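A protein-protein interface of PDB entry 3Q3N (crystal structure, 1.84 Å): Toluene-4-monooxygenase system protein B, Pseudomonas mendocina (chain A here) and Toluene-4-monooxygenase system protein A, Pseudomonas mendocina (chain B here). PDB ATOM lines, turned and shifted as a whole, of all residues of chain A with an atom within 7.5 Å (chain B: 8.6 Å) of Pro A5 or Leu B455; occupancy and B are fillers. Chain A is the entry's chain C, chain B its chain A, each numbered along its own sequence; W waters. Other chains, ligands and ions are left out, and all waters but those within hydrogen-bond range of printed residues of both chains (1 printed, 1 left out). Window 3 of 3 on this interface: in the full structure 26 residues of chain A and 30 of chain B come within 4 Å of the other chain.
NE2 of His B427 is in hydrogen-bond range of O of Thr A75 (2.7 Å). The side-chain hydroxyl of Ser B395 is in hydrogen-bond range of the backbone NH of Leu A18, at 3.4 Å. N of Leu A18 sits at hydrogen-bond distance from O of Leu B393, 2.9 Å away.
O of Pro A5 sits at hydrogen-bond distance from N of Thr A75, 2.7 Å away. A ring nitrogen (ND1) of His A7 sits at hydrogen-bond distance from the backbone carbonyl oxygen of Thr A75. The side-chain amide nitrogen (ND2) of Asn A73 lies within hydrogen-bond range of the side-chain carboxylate (OE2) of Glu A76. The backbone NH (N) of His A7 lies within hydrogen-bond range of the backbone carbonyl oxygen (O) of Glu A76 (3.2 Å).
Leu B455 touches Pro A5 (CD2 to CB, 3.997 Å). His A7 touches Ser B395. His A7 touches His B427 (ND1 to NE2, 3.9 Å). Thr A75 touches Leu B425. CG of Glu A76 touches CD2 of Leu B425, 3.8 Å away. Val A77 touches His B427 (CG2 to CE1, 3.5 Å).
Printed residues of chain B within 4 Å of Pro A5: Leu B455 (3.997 Å). Printed residues of chain A within 4 Å of Leu B455: Pro A5 (3.997 Å). No residue of chain B comes within 4 Å of Val A6. Of the printed residues of chain B, Thr A75 touches Leu B425 and His B427. Of the printed residues of chain B, His A7 touches Ser B395 (2.8 Å) and His B427 (3.9 Å). Printed residues of chain B within 4 Å of Val A77: His B427. Val A21 touches none of the printed residues of chain B. The nearest printed residue of chain B that does not touch Pro A5 is Val B451 (7.7 Å). The nearest printed residue of chain A that does not touch Ser B395 is Val A6 (5.6 Å).
Hydrophobic or aromatic side chains of chain A that line the printed part of chain B: Pro A5, His A7, Leu A18 and Val A77. Printed residues of chain B that touch a printed residue of chain A: Leu B393, Ser B395, Leu B425, His B427 and Leu B455. Among the printed residues, no Asp or Glu carboxylate lies within 4 Å of a Lys or Arg side-chain nitrogen of the other chain.
Water W1 lies within hydrogen-bond range of the backbone carbonyl oxygen (O) of Leu B425 and the side-chain hydroxyl (OG1) of Thr A75.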
ATOM      1  N   SER A   2     -23.828   6.899  -8.105  1.00  0.00           N
ATOM      2  CA  SER A   2     -24.578   7.379  -9.258  1.00  0.00           C
ATOM      3  C   SER A   2     -23.706   7.373 -10.517  1.00  0.00           C
ATOM      4  O   SER A   2     -22.557   7.829 -10.488  1.00  0.00           O
ATOM      5  CB  SER A   2     -25.116   8.787  -8.986  1.00  0.00           C
ATOM      6  OG  SER A   2     -26.186   9.106  -9.856  1.00  0.00           O
ATOM      7  N   ALA A   3     -24.261   6.853 -11.612  1.00  0.00           N
ATOM      8  CA  ALA A   3     -23.551   6.747 -12.889  1.00  0.00           C
ATOM      9  C   ALA A   3     -22.968   8.084 -13.345  1.00  0.00           C
ATOM     10  O   ALA A   3     -23.590   9.134 -13.188  1.00  0.00           O
ATOM     11  CB  ALA A   3     -24.466   6.180 -13.964  1.00  0.00           C
ATOM     12  N   PHE A   4     -21.775   8.035 -13.924  1.00  0.00           N
ATOM     13  CA  PHE A   4     -21.070   9.247 -14.308  1.00  0.00           C
ATOM     14  C   PHE A   4     -20.170   8.983 -15.506  1.00  0.00           C
ATOM     15  O   PHE A   4     -19.067   8.464 -15.351  1.00  0.00           O
ATOM     16  CB  PHE A   4     -20.236   9.754 -13.125  1.00  0.00           C
ATOM     17  CG  PHE A   4     -19.694  11.137 -13.317  1.00  0.00           C
ATOM     18  CD1 PHE A   4     -20.279  12.218 -12.676  1.00  0.00           C
ATOM     19  CD2 PHE A   4     -18.603  11.362 -14.140  1.00  0.00           C
ATOM     20  CE1 PHE A   4     -19.781  13.493 -12.848  1.00  0.00           C
ATOM     21  CE2 PHE A   4     -18.101  12.635 -14.315  1.00  0.00           C
ATOM     22  CZ  PHE A   4     -18.691  13.701 -13.672  1.00  0.00           C
ATOM     23  N   PRO A   5     -20.641   9.339 -16.708  1.00  0.00           N
ATOM     24  CA  PRO A   5     -19.880   9.095 -17.935  1.00  0.00           C
ATOM     25  C   PRO A   5     -18.699  10.038 -18.094  1.00  0.00           C
ATOM     26  O   PRO A   5     -18.831  11.251 -17.896  1.00  0.00           O
ATOM     27  CB  PRO A   5     -20.901   9.379 -19.035  1.00  0.00           C
ATOM     28  CG  PRO A   5     -21.803  10.399 -18.441  1.00  0.00           C
ATOM     29  CD  PRO A   5     -21.916  10.027 -16.979  1.00  0.00           C
ATOM     30  N   VAL A   6     -17.550   9.474 -18.449  1.00  0.00           N
ATOM     31  CA  VAL A   6     -16.386  10.256 -18.853  1.00  0.00           C
ATOM     32  C   VAL A   6     -15.805   9.668 -20.137  1.00  0.00           C
ATOM     33  O   VAL A   6     -16.158   8.556 -20.535  1.00  0.00           O
ATOM     34  CB  VAL A   6     -15.295  10.251 -17.767  1.00  0.00           C
ATOM     35  CG1 VAL A   6     -15.872  10.723 -16.447  1.00  0.00           C
ATOM     36  CG2 VAL A   6     -14.714   8.851 -17.609  1.00  0.00           C
ATOM     37  N   HIS A   7     -14.925  10.420 -20.791  1.00  0.00           N
ATOM     38  CA  HIS A   7     -14.187   9.894 -21.932  1.00  0.00           C
ATOM     39  C   HIS A   7     -12.720   9.812 -21.536  1.00  0.00           C
ATOM     40  O   HIS A   7     -12.120  10.816 -21.154  1.00  0.00           O
ATOM     41  CB  HIS A   7     -14.386  10.771 -23.172  1.00  0.00           C
ATOM     42  CG  HIS A   7     -15.783  10.736 -23.712  1.00  0.00           C
ATOM     43  ND1 HIS A   7     -16.683  11.763 -23.522  1.00  0.00           N
ATOM     44  CD2 HIS A   7     -16.441   9.786 -24.420  1.00  0.00           C
ATOM     45  CE1 HIS A   7     -17.832  11.451 -24.096  1.00  0.00           C
ATOM     46  NE2 HIS A   7     -17.710  10.258 -24.651  1.00  0.00           N
ATOM     47  N   LEU A  18     -15.438   5.725 -24.123  1.00  0.00           N
ATOM     48  CA  LEU A  18     -16.459   6.008 -23.117  1.00  0.00           C
ATOM     49  C   LEU A  18     -16.335   5.023 -21.961  1.00  0.00           C
ATOM     50  O   LEU A  18     -16.394   3.814 -22.158  1.00  0.00           O
ATOM     51  CB  LEU A  18     -17.868   5.914 -23.710  1.00  0.00           C
ATOM     52  CG  LEU A  18     -18.991   6.004 -22.672  1.00  0.00           C
ATOM     53  CD1 LEU A  18     -19.126   7.438 -22.128  1.00  0.00           C
ATOM     54  CD2 LEU A  18     -20.316   5.512 -23.249  1.00  0.00           C
ATOM     55  N   VAL A  19     -16.147   5.543 -20.753  1.00  0.00           N
ATOM     56  CA  VAL A  19     -16.142   4.712 -19.560  1.00  0.00           C
ATOM     57  C   VAL A  19     -17.055   5.356 -18.538  1.00  0.00           C
ATOM     58  O   VAL A  19     -16.868   6.512 -18.170  1.00  0.00           O
ATOM     59  CB  VAL A  19     -14.734   4.571 -18.951  1.00  0.00           C
ATOM     60  CG1 VAL A  19     -14.789   3.723 -17.688  1.00  0.00           C
ATOM     61  CG2 VAL A  19     -13.772   3.963 -19.967  1.00  0.00           C
ATOM     62  N   VAL A  20     -18.060   4.616 -18.100  1.00  0.00           N
ATOM     63  CA  VAL A  20     -18.982   5.131 -17.102  1.00  0.00           C
ATOM     64  C   VAL A  20     -18.490   4.767 -15.710  1.00  0.00           C
ATOM     65  O   VAL A  20     -18.405   3.590 -15.360  1.00  0.00           O
ATOM     66  CB  VAL A  20     -20.400   4.579 -17.324  1.00  0.00           C
ATOM     67  CG1 VAL A  20     -21.310   4.933 -16.150  1.00  0.00           C
ATOM     68  CG2 VAL A  20     -20.963   5.094 -18.644  1.00  0.00           C
ATOM     69  N   VAL A  21     -18.148   5.781 -14.926  1.00  0.00           N
ATOM     70  CA  VAL A  21     -17.701   5.565 -13.562  1.00  0.00           C
ATOM     71  C   VAL A  21     -18.809   5.969 -12.595  1.00  0.00           C
ATOM     72  O   VAL A  21     -19.932   6.260 -13.017  1.00  0.00           O
ATOM     73  CB  VAL A  21     -16.416   6.359 -13.255  1.00  0.00           C
ATOM     74  CG1 VAL A  21     -15.335   6.017 -14.266  1.00  0.00           C
ATOM     75  CG2 VAL A  21     -16.694   7.858 -13.250  1.00  0.00           C
ATOM     76  N   ASP A  22     -18.498   5.973 -11.303  1.00  0.00           N
ATOM     77  CA  ASP A  22     -19.470   6.376 -10.295  1.00  0.00           C
ATOM     78  C   ASP A  22     -19.112   7.721  -9.664  1.00  0.00           C
ATOM     79  O   ASP A  22     -17.939   8.034  -9.454  1.00  0.00           O
ATOM     80  CB  ASP A  22     -19.601   5.309  -9.208  1.00  0.00           C
ATOM     81  CG  ASP A  22     -20.732   5.601  -8.246  1.00  0.00           C
ATOM     82  OD1 ASP A  22     -20.521   6.375  -7.287  1.00  0.00           O
ATOM     83  OD2 ASP A  22     -21.839   5.063  -8.454  1.00  0.00           O
ATOM     84  N   LEU A  23     -20.136   8.508  -9.355  1.00  0.00           N
ATOM     85  CA  LEU A  23     -19.956   9.813  -8.728  1.00  0.00           C
ATOM     86  C   LEU A  23     -19.044   9.749  -7.498  1.00  0.00           C
ATOM     87  O   LEU A  23     -18.358  10.717  -7.171  1.00  0.00           O
ATOM     88  CB  LEU A  23     -21.321  10.390  -8.346  1.00  0.00           C
ATOM     89  CG  LEU A  23     -21.397  11.836  -7.866  1.00  0.00           C
ATOM     90  CD1 LEU A  23     -20.917  12.787  -8.950  1.00  0.00           C
ATOM     91  CD2 LEU A  23     -22.821  12.165  -7.457  1.00  0.00           C
ATOM     92  N   ILE A  67     -14.579  11.502  -7.781  1.00  0.00           N
ATOM     93  CA  ILE A  67     -14.943  12.306  -8.941  1.00  0.00           C
ATOM     94  C   ILE A  67     -15.878  13.436  -8.509  1.00  0.00           C
ATOM     95  O   ILE A  67     -15.859  14.519  -9.084  1.00  0.00           O
ATOM     96  CB  ILE A  67     -15.547  11.463 -10.100  1.00  0.00           C
ATOM     97  CG1 ILE A  67     -17.018  11.142  -9.850  1.00  0.00           C
ATOM     98  CG2 ILE A  67     -14.742  10.196 -10.334  1.00  0.00           C
ATOM     99  CD1 ILE A  67     -17.954  12.133 -10.481  1.00  0.00           C
ATOM    100  N   ASN A  73     -17.040  17.506 -14.807  1.00  0.00           N
ATOM    101  CA  ASN A  73     -18.411  17.414 -15.294  1.00  0.00           C
ATOM    102  C   ASN A  73     -18.617  16.153 -16.124  1.00  0.00           C
ATOM    103  O   ASN A  73     -17.665  15.622 -16.697  1.00  0.00           O
ATOM    104  CB  ASN A  73     -18.768  18.647 -16.121  1.00  0.00           C
ATOM    105  CG  ASN A  73     -18.656  19.931 -15.316  1.00  0.00           C
ATOM    106  OD1 ASN A  73     -18.971  19.953 -14.133  1.00  0.00           O
ATOM    107  ND2 ASN A  73     -18.197  20.998 -15.954  1.00  0.00           N
ATOM    108  N   PRO A  74     -19.863  15.670 -16.202  1.00  0.00           N
ATOM    109  CA  PRO A  74     -20.080  14.482 -17.030  1.00  0.00           C
ATOM    110  C   PRO A  74     -19.600  14.715 -18.459  1.00  0.00           C
ATOM    111  O   PRO A  74     -19.655  15.837 -18.968  1.00  0.00           O
ATOM    112  CB  PRO A  74     -21.599  14.304 -16.992  1.00  0.00           C
ATOM    113  CG  PRO A  74     -22.016  14.921 -15.714  1.00  0.00           C
ATOM    114  CD  PRO A  74     -21.092  16.095 -15.510  1.00  0.00           C
ATOM    115  N   THR A  75     -19.111  13.650 -19.080  1.00  0.00           N
ATOM    116  CA  THR A  75     -18.647  13.656 -20.470  1.00  0.00           C
ATOM    117  C   THR A  75     -17.400  14.505 -20.748  1.00  0.00           C
ATOM    118  O   THR A  75     -17.017  14.667 -21.905  1.00  0.00           O
ATOM    119  CB  THR A  75     -19.772  14.015 -21.483  1.00  0.00           C
ATOM    120  OG1 THR A  75     -19.953  15.433 -21.538  1.00  0.00           O
ATOM    121  CG2 THR A  75     -21.080  13.341 -21.098  1.00  0.00           C
ATOM    122  N   GLU A  76     -16.770  15.041 -19.703  1.00  0.00           N
ATOM    123  CA  GLU A  76     -15.457  15.666 -19.867  1.00  0.00           C
ATOM    124  C   GLU A  76     -14.395  14.580 -20.109  1.00  0.00           C
ATOM    125  O   GLU A  76     -14.593  13.413 -19.764  1.00  0.00           O
ATOM    126  CB  GLU A  76     -15.100  16.557 -18.659  1.00  0.00           C
ATOM    127  CG  GLU A  76     -15.853  17.895 -18.652  1.00  0.00           C
ATOM    128  CD  GLU A  76     -15.511  18.818 -17.469  1.00  0.00           C
ATOM    129  OE1 GLU A  76     -14.819  18.386 -16.517  1.00  0.00           O
ATOM    130  OE2 GLU A  76     -15.956  19.989 -17.493  1.00  0.00           O
ATOM    131  N   VAL A  77     -13.277  14.966 -20.715  1.00  0.00           N
ATOM    132  CA  VAL A  77     -12.208  14.022 -21.055  1.00  0.00           C
ATOM    133  C   VAL A  77     -11.104  13.953 -19.981  1.00  0.00           C
ATOM    134  O   VAL A  77     -10.637  14.993 -19.505  1.00  0.00           O
ATOM    135  CB  VAL A  77     -11.553  14.407 -22.400  1.00  0.00           C
ATOM    136  CG1 VAL A  77     -10.571  13.329 -22.856  1.00  0.00           C
ATOM    137  CG2 VAL A  77     -12.616  14.666 -23.460  1.00  0.00           C
ATOM    138  N   LEU B 393     -18.050   1.616 -25.727  1.00  0.00           N
ATOM    139  CA  LEU B 393     -18.046   2.423 -26.946  1.00  0.00           C
ATOM    140  C   LEU B 393     -16.766   3.240 -27.059  1.00  0.00           C
ATOM    141  O   LEU B 393     -16.193   3.647 -26.053  1.00  0.00           O
ATOM    142  CB  LEU B 393     -19.220   3.402 -26.943  1.00  0.00           C
ATOM    143  CG  LEU B 393     -20.656   2.901 -27.036  1.00  0.00           C
ATOM    144  CD1 LEU B 393     -21.611   4.029 -26.705  1.00  0.00           C
ATOM    145  CD2 LEU B 393     -20.924   2.402 -28.406  1.00  0.00           C
ATOM    146  N   SER B 395     -15.066   6.834 -27.877  1.00  0.00           N
ATOM    147  CA  SER B 395     -15.465   8.229 -27.937  1.00  0.00           C
ATOM    148  C   SER B 395     -15.411   8.665 -29.407  1.00  0.00           C
ATOM    149  O   SER B 395     -14.477   8.305 -30.129  1.00  0.00           O
ATOM    150  CB  SER B 395     -14.530   9.078 -27.073  1.00  0.00           C
ATOM    151  OG  SER B 395     -14.354   8.485 -25.786  1.00  0.00           O
ATOM    152  N   LEU B 425     -21.484  20.310 -24.386  1.00  0.00           N
ATOM    153  CA  LEU B 425     -20.061  20.025 -24.538  1.00  0.00           C
ATOM    154  C   LEU B 425     -19.792  19.112 -25.741  1.00  0.00           C
ATOM    155  O   LEU B 425     -20.250  17.967 -25.761  1.00  0.00           O
ATOM    156  CB  LEU B 425     -19.523  19.374 -23.262  1.00  0.00           C
ATOM    157  CG  LEU B 425     -18.027  19.078 -23.243  1.00  0.00           C
ATOM    158  CD1 LEU B 425     -17.246  20.377 -23.458  1.00  0.00           C
ATOM    159  CD2 LEU B 425     -17.630  18.425 -21.929  1.00  0.00           C
ATOM    160  N   HIS B 427     -16.911  17.343 -28.597  1.00  0.00           N
ATOM    161  CA  HIS B 427     -15.532  16.856 -28.665  1.00  0.00           C
ATOM    162  C   HIS B 427     -15.117  16.599 -30.113  1.00  0.00           C
ATOM    163  O   HIS B 427     -15.841  15.926 -30.849  1.00  0.00           O
ATOM    164  CB  HIS B 427     -15.409  15.544 -27.883  1.00  0.00           C
ATOM    165  CG  HIS B 427     -15.744  15.673 -26.430  1.00  0.00           C
ATOM    166  ND1 HIS B 427     -14.980  16.413 -25.553  1.00  0.00           N
ATOM    167  CD2 HIS B 427     -16.763  15.161 -25.701  1.00  0.00           C
ATOM    168  CE1 HIS B 427     -15.511  16.347 -24.343  1.00  0.00           C
ATOM    169  NE2 HIS B 427     -16.589  15.586 -24.406  1.00  0.00           N
ATOM    170  N   MET B 448     -26.565  15.082 -32.981  1.00  0.00           N
ATOM    171  CA  MET B 448     -26.044  14.212 -31.935  1.00  0.00           C
ATOM    172  C   MET B 448     -25.377  13.012 -32.576  1.00  0.00           C
ATOM    173  O   MET B 448     -25.978  12.332 -33.412  1.00  0.00           O
ATOM    174  CB  MET B 448     -27.164  13.735 -31.007  1.00  0.00           C
ATOM    175  CG  MET B 448     -27.902  14.858 -30.304  1.00  0.00           C
ATOM    176  SD  MET B 448     -29.290  14.224 -29.351  1.00  0.00           S
ATOM    177  CE  MET B 448     -28.440  13.183 -28.163  1.00  0.00           C
ATOM    178  N   ASN B 449     -24.131  12.750 -32.197  1.00  0.00           N
ATOM    179  CA  ASN B 449     -23.425  11.595 -32.740  1.00  0.00           C
ATOM    180  C   ASN B 449     -23.885  10.339 -32.006  1.00  0.00           C
ATOM    181  O   ASN B 449     -24.663  10.417 -31.049  1.00  0.00           O
ATOM    182  CB  ASN B 449     -21.895  11.782 -32.746  1.00  0.00           C
ATOM    183  CG  ASN B 449     -21.270  11.708 -31.365  1.00  0.00           C
ATOM    184  OD1 ASN B 449     -21.839  11.142 -30.437  1.00  0.00           O
ATOM    185  ND2 ASN B 449     -20.074  12.275 -31.234  1.00  0.00           N
ATOM    186  N   ILE B 450     -23.417   9.186 -32.451  1.00  0.00           N
ATOM    187  CA  ILE B 450     -23.958   7.917 -31.957  1.00  0.00           C
ATOM    188  C   ILE B 450     -23.786   7.741 -30.444  1.00  0.00           C
ATOM    189  O   ILE B 450     -24.669   7.193 -29.767  1.00  0.00           O
ATOM    190  CB  ILE B 450     -23.353   6.718 -32.746  1.00  0.00           C
ATOM    191  CG1 ILE B 450     -24.095   5.421 -32.430  1.00  0.00           C
ATOM    192  CG2 ILE B 450     -21.861   6.578 -32.488  1.00  0.00           C
ATOM    193  CD1 ILE B 450     -25.411   5.313 -33.128  1.00  0.00           C
ATOM    194  N   VAL B 451     -22.659   8.209 -29.918  1.00  0.00           N
ATOM    195  CA  VAL B 451     -22.390   8.142 -28.481  1.00  0.00           C
ATOM    196  C   VAL B 451     -23.245   9.144 -27.688  1.00  0.00           C
ATOM    197  O   VAL B 451     -23.720   8.830 -26.594  1.00  0.00           O
ATOM    198  CB  VAL B 451     -20.883   8.344 -28.183  1.00  0.00           C
ATOM    199  CG1 VAL B 451     -20.627   8.353 -26.691  1.00  0.00           C
ATOM    200  CG2 VAL B 451     -20.052   7.252 -28.866  1.00  0.00           C
ATOM    201  N   ASP B 452     -23.443  10.343 -28.236  1.00  0.00           N
ATOM    202  CA  ASP B 452     -24.397  11.292 -27.659  1.00  0.00           C
ATOM    203  C   ASP B 452     -25.782  10.652 -27.528  1.00  0.00           C
ATOM    204  O   ASP B 452     -26.457  10.816 -26.515  1.00  0.00           O
ATOM    205  CB  ASP B 452     -24.532  12.537 -28.538  1.00  0.00           C
ATOM    206  CG  ASP B 452     -23.250  13.341 -28.633  1.00  0.00           C
ATOM    207  OD1 ASP B 452     -22.484  13.387 -27.649  1.00  0.00           O
ATOM    208  OD2 ASP B 452     -23.017  13.937 -29.705  1.00  0.00           O
ATOM    209  N   ARG B 453     -26.211   9.947 -28.571  1.00  0.00           N
ATOM    210  CA  ARG B 453     -27.507   9.262 -28.572  1.00  0.00           C
ATOM    211  C   ARG B 453     -27.570   8.129 -27.540  1.00  0.00           C
ATOM    212  O   ARG B 453     -28.591   7.935 -26.867  1.00  0.00           O
ATOM    213  CB  ARG B 453     -27.810   8.703 -29.975  1.00  0.00           C
ATOM    214  CG  ARG B 453     -27.859   9.779 -31.062  1.00  0.00           C
ATOM    215  CD  ARG B 453     -28.105   9.193 -32.448  1.00  0.00           C
ATOM    216  NE  ARG B 453     -27.753  10.163 -33.488  1.00  0.00           N
ATOM    217  CZ  ARG B 453     -27.985  10.000 -34.783  1.00  0.00           C
ATOM    218  NH1 ARG B 453     -28.584   8.897 -35.225  1.00  0.00           N
ATOM    219  NH2 ARG B 453     -27.620  10.949 -35.640  1.00  0.00           N
ATOM    220  N   PHE B 454     -26.485   7.364 -27.443  1.00  0.00           N
ATOM    221  CA  PHE B 454     -26.381   6.286 -26.460  1.00  0.00           C
ATOM    222  C   PHE B 454     -26.548   6.860 -25.052  1.00  0.00           C
ATOM    223  O   PHE B 454     -27.296   6.332 -24.234  1.00  0.00           O
ATOM    224  CB  PHE B 454     -25.018   5.594 -26.607  1.00  0.00           C
ATOM    225  CG  PHE B 454     -24.853   4.368 -25.757  1.00  0.00           C
ATOM    226  CD1 PHE B 454     -25.253   3.122 -26.227  1.00  0.00           C
ATOM    227  CD2 PHE B 454     -24.283   4.451 -24.499  1.00  0.00           C
ATOM    228  CE1 PHE B 454     -25.104   1.987 -25.450  1.00  0.00           C
ATOM    229  CE2 PHE B 454     -24.127   3.314 -23.719  1.00  0.00           C
ATOM    230  CZ  PHE B 454     -24.538   2.081 -24.199  1.00  0.00           C
ATOM    231  N   LEU B 455     -25.851   7.960 -24.785  1.00  0.00           N
ATOM    232  CA  LEU B 455     -25.890   8.596 -23.475  1.00  0.00           C
ATOM    233  C   LEU B 455     -27.216   9.293 -23.198  1.00  0.00           C
ATOM    234  O   LEU B 455     -27.582   9.483 -22.041  1.00  0.00           O
ATOM    235  CB  LEU B 455     -24.746   9.597 -23.323  1.00  0.00           C
ATOM    236  CG  LEU B 455     -23.339   9.011 -23.227  1.00  0.00           C
ATOM    237  CD1 LEU B 455     -22.314  10.135 -23.165  1.00  0.00           C
ATOM    238  CD2 LEU B 455     -23.228   8.091 -22.018  1.00  0.00           C
ATOM    239  N   ALA B 456     -27.926   9.677 -24.256  1.00  0.00           N
ATOM    240  CA  ALA B 456     -29.209  10.367 -24.114  1.00  0.00           C
ATOM    241  C   ALA B 456     -30.372   9.395 -23.932  1.00  0.00           C
ATOM    242  O   ALA B 456     -31.504   9.814 -23.693  1.00  0.00           O
ATOM    243  CB  ALA B 456     -29.468  11.259 -25.318  1.00  0.00           C
ATOM    244  N   GLY B 457     -30.096   8.100 -24.066  1.00  0.00           N
ATOM    245  CA  GLY B 457     -31.113   7.079 -23.844  1.00  0.00           C
ATOM    246  C   GLY B 457     -31.873   6.677 -25.098  1.00  0.00           C
ATOM    247  O   GLY B 457     -32.886   5.983 -25.022  1.00  0.00           O
ATOM    248  N   GLN B 458     -31.387   7.107 -26.258  1.00  0.00           N
ATOM    249  CA  GLN B 458     -32.060   6.808 -27.522  1.00  0.00           C
ATOM    250  C   GLN B 458     -31.749   5.403 -28.040  1.00  0.00           C
ATOM    251  O   GLN B 458     -32.390   4.926 -28.979  1.00  0.00           O
ATOM    252  CB  GLN B 458     -31.674   7.829 -28.594  1.00  0.00           C
ATOM    253  CG  GLN B 458     -31.925   9.271 -28.204  1.00  0.00           C
ATOM    254  CD  GLN B 458     -31.439  10.245 -29.261  1.00  0.00           C
ATOM    255  OE1 GLN B 458     -31.304  11.434 -28.995  1.00  0.00           O
ATOM    256  NE2 GLN B 458     -31.177   9.741 -30.469  1.00  0.00           N
ATOM    257  N   ILE B 459     -30.752   4.753 -27.446  1.00  0.00           N
ATOM    258  CA  ILE B 459     -30.360   3.411 -27.876  1.00  0.00           C
ATOM    259  C   ILE B 459     -30.669   2.403 -26.773  1.00  0.00           C
ATOM    260  O   ILE B 459     -30.043   2.415 -25.713  1.00  0.00           O
ATOM    261  CB  ILE B 459     -28.862   3.356 -28.281  1.00  0.00           C
ATOM    262  CG1 ILE B 459     -28.595   4.331 -29.433  1.00  0.00           C
ATOM    263  CG2 ILE B 459     -28.447   1.928 -28.653  1.00  0.00           C
ATOM    264  CD1 ILE B 459     -27.121   4.480 -29.805  1.00  0.00           C
ATOM    265  N   GLN B 460     -31.653   1.544 -27.022  1.00  0.00           N
ATOM    266  CA  GLN B 460     -32.122   0.606 -26.007  1.00  0.00           C
ATOM    267  C   GLN B 460     -32.184  -0.822 -26.547  1.00  0.00           C
ATOM    268  O   GLN B 460     -32.665  -1.050 -27.653  1.00  0.00           O
ATOM    269  CB  GLN B 460     -33.492   1.044 -25.479  1.00  0.00           C
ATOM    270  CG  GLN B 460     -33.495   2.452 -24.881  1.00  0.00           C
ATOM    271  CD  GLN B 460     -32.764   2.522 -23.558  1.00  0.00           C
ATOM    272  OE1 GLN B 460     -32.524   1.498 -22.926  1.00  0.00           O
ATOM    273  NE2 GLN B 460     -32.405   3.737 -23.129  1.00  0.00           N
ATOM    274  N   MET B 462     -29.100  -0.431 -23.513  1.00  0.00           N
ATOM    275  CA  MET B 462     -27.772   0.170 -23.545  1.00  0.00           C
ATOM    276  C   MET B 462     -26.684  -0.891 -23.404  1.00  0.00           C
ATOM    277  O   MET B 462     -26.026  -0.995 -22.367  1.00  0.00           O
ATOM    278  CB  MET B 462     -27.657   1.243 -22.454  1.00  0.00           C
ATOM    279  CG  MET B 462     -28.455   2.502 -22.788  1.00  0.00           C
ATOM    280  SD  MET B 462     -28.515   3.724 -21.461  1.00  0.00           S
ATOM    281  CE  MET B 462     -26.831   4.333 -21.448  1.00  0.00           C
HETATM  282  O   HOH W   1     -21.602  16.044 -24.114  1.00  0.00           O
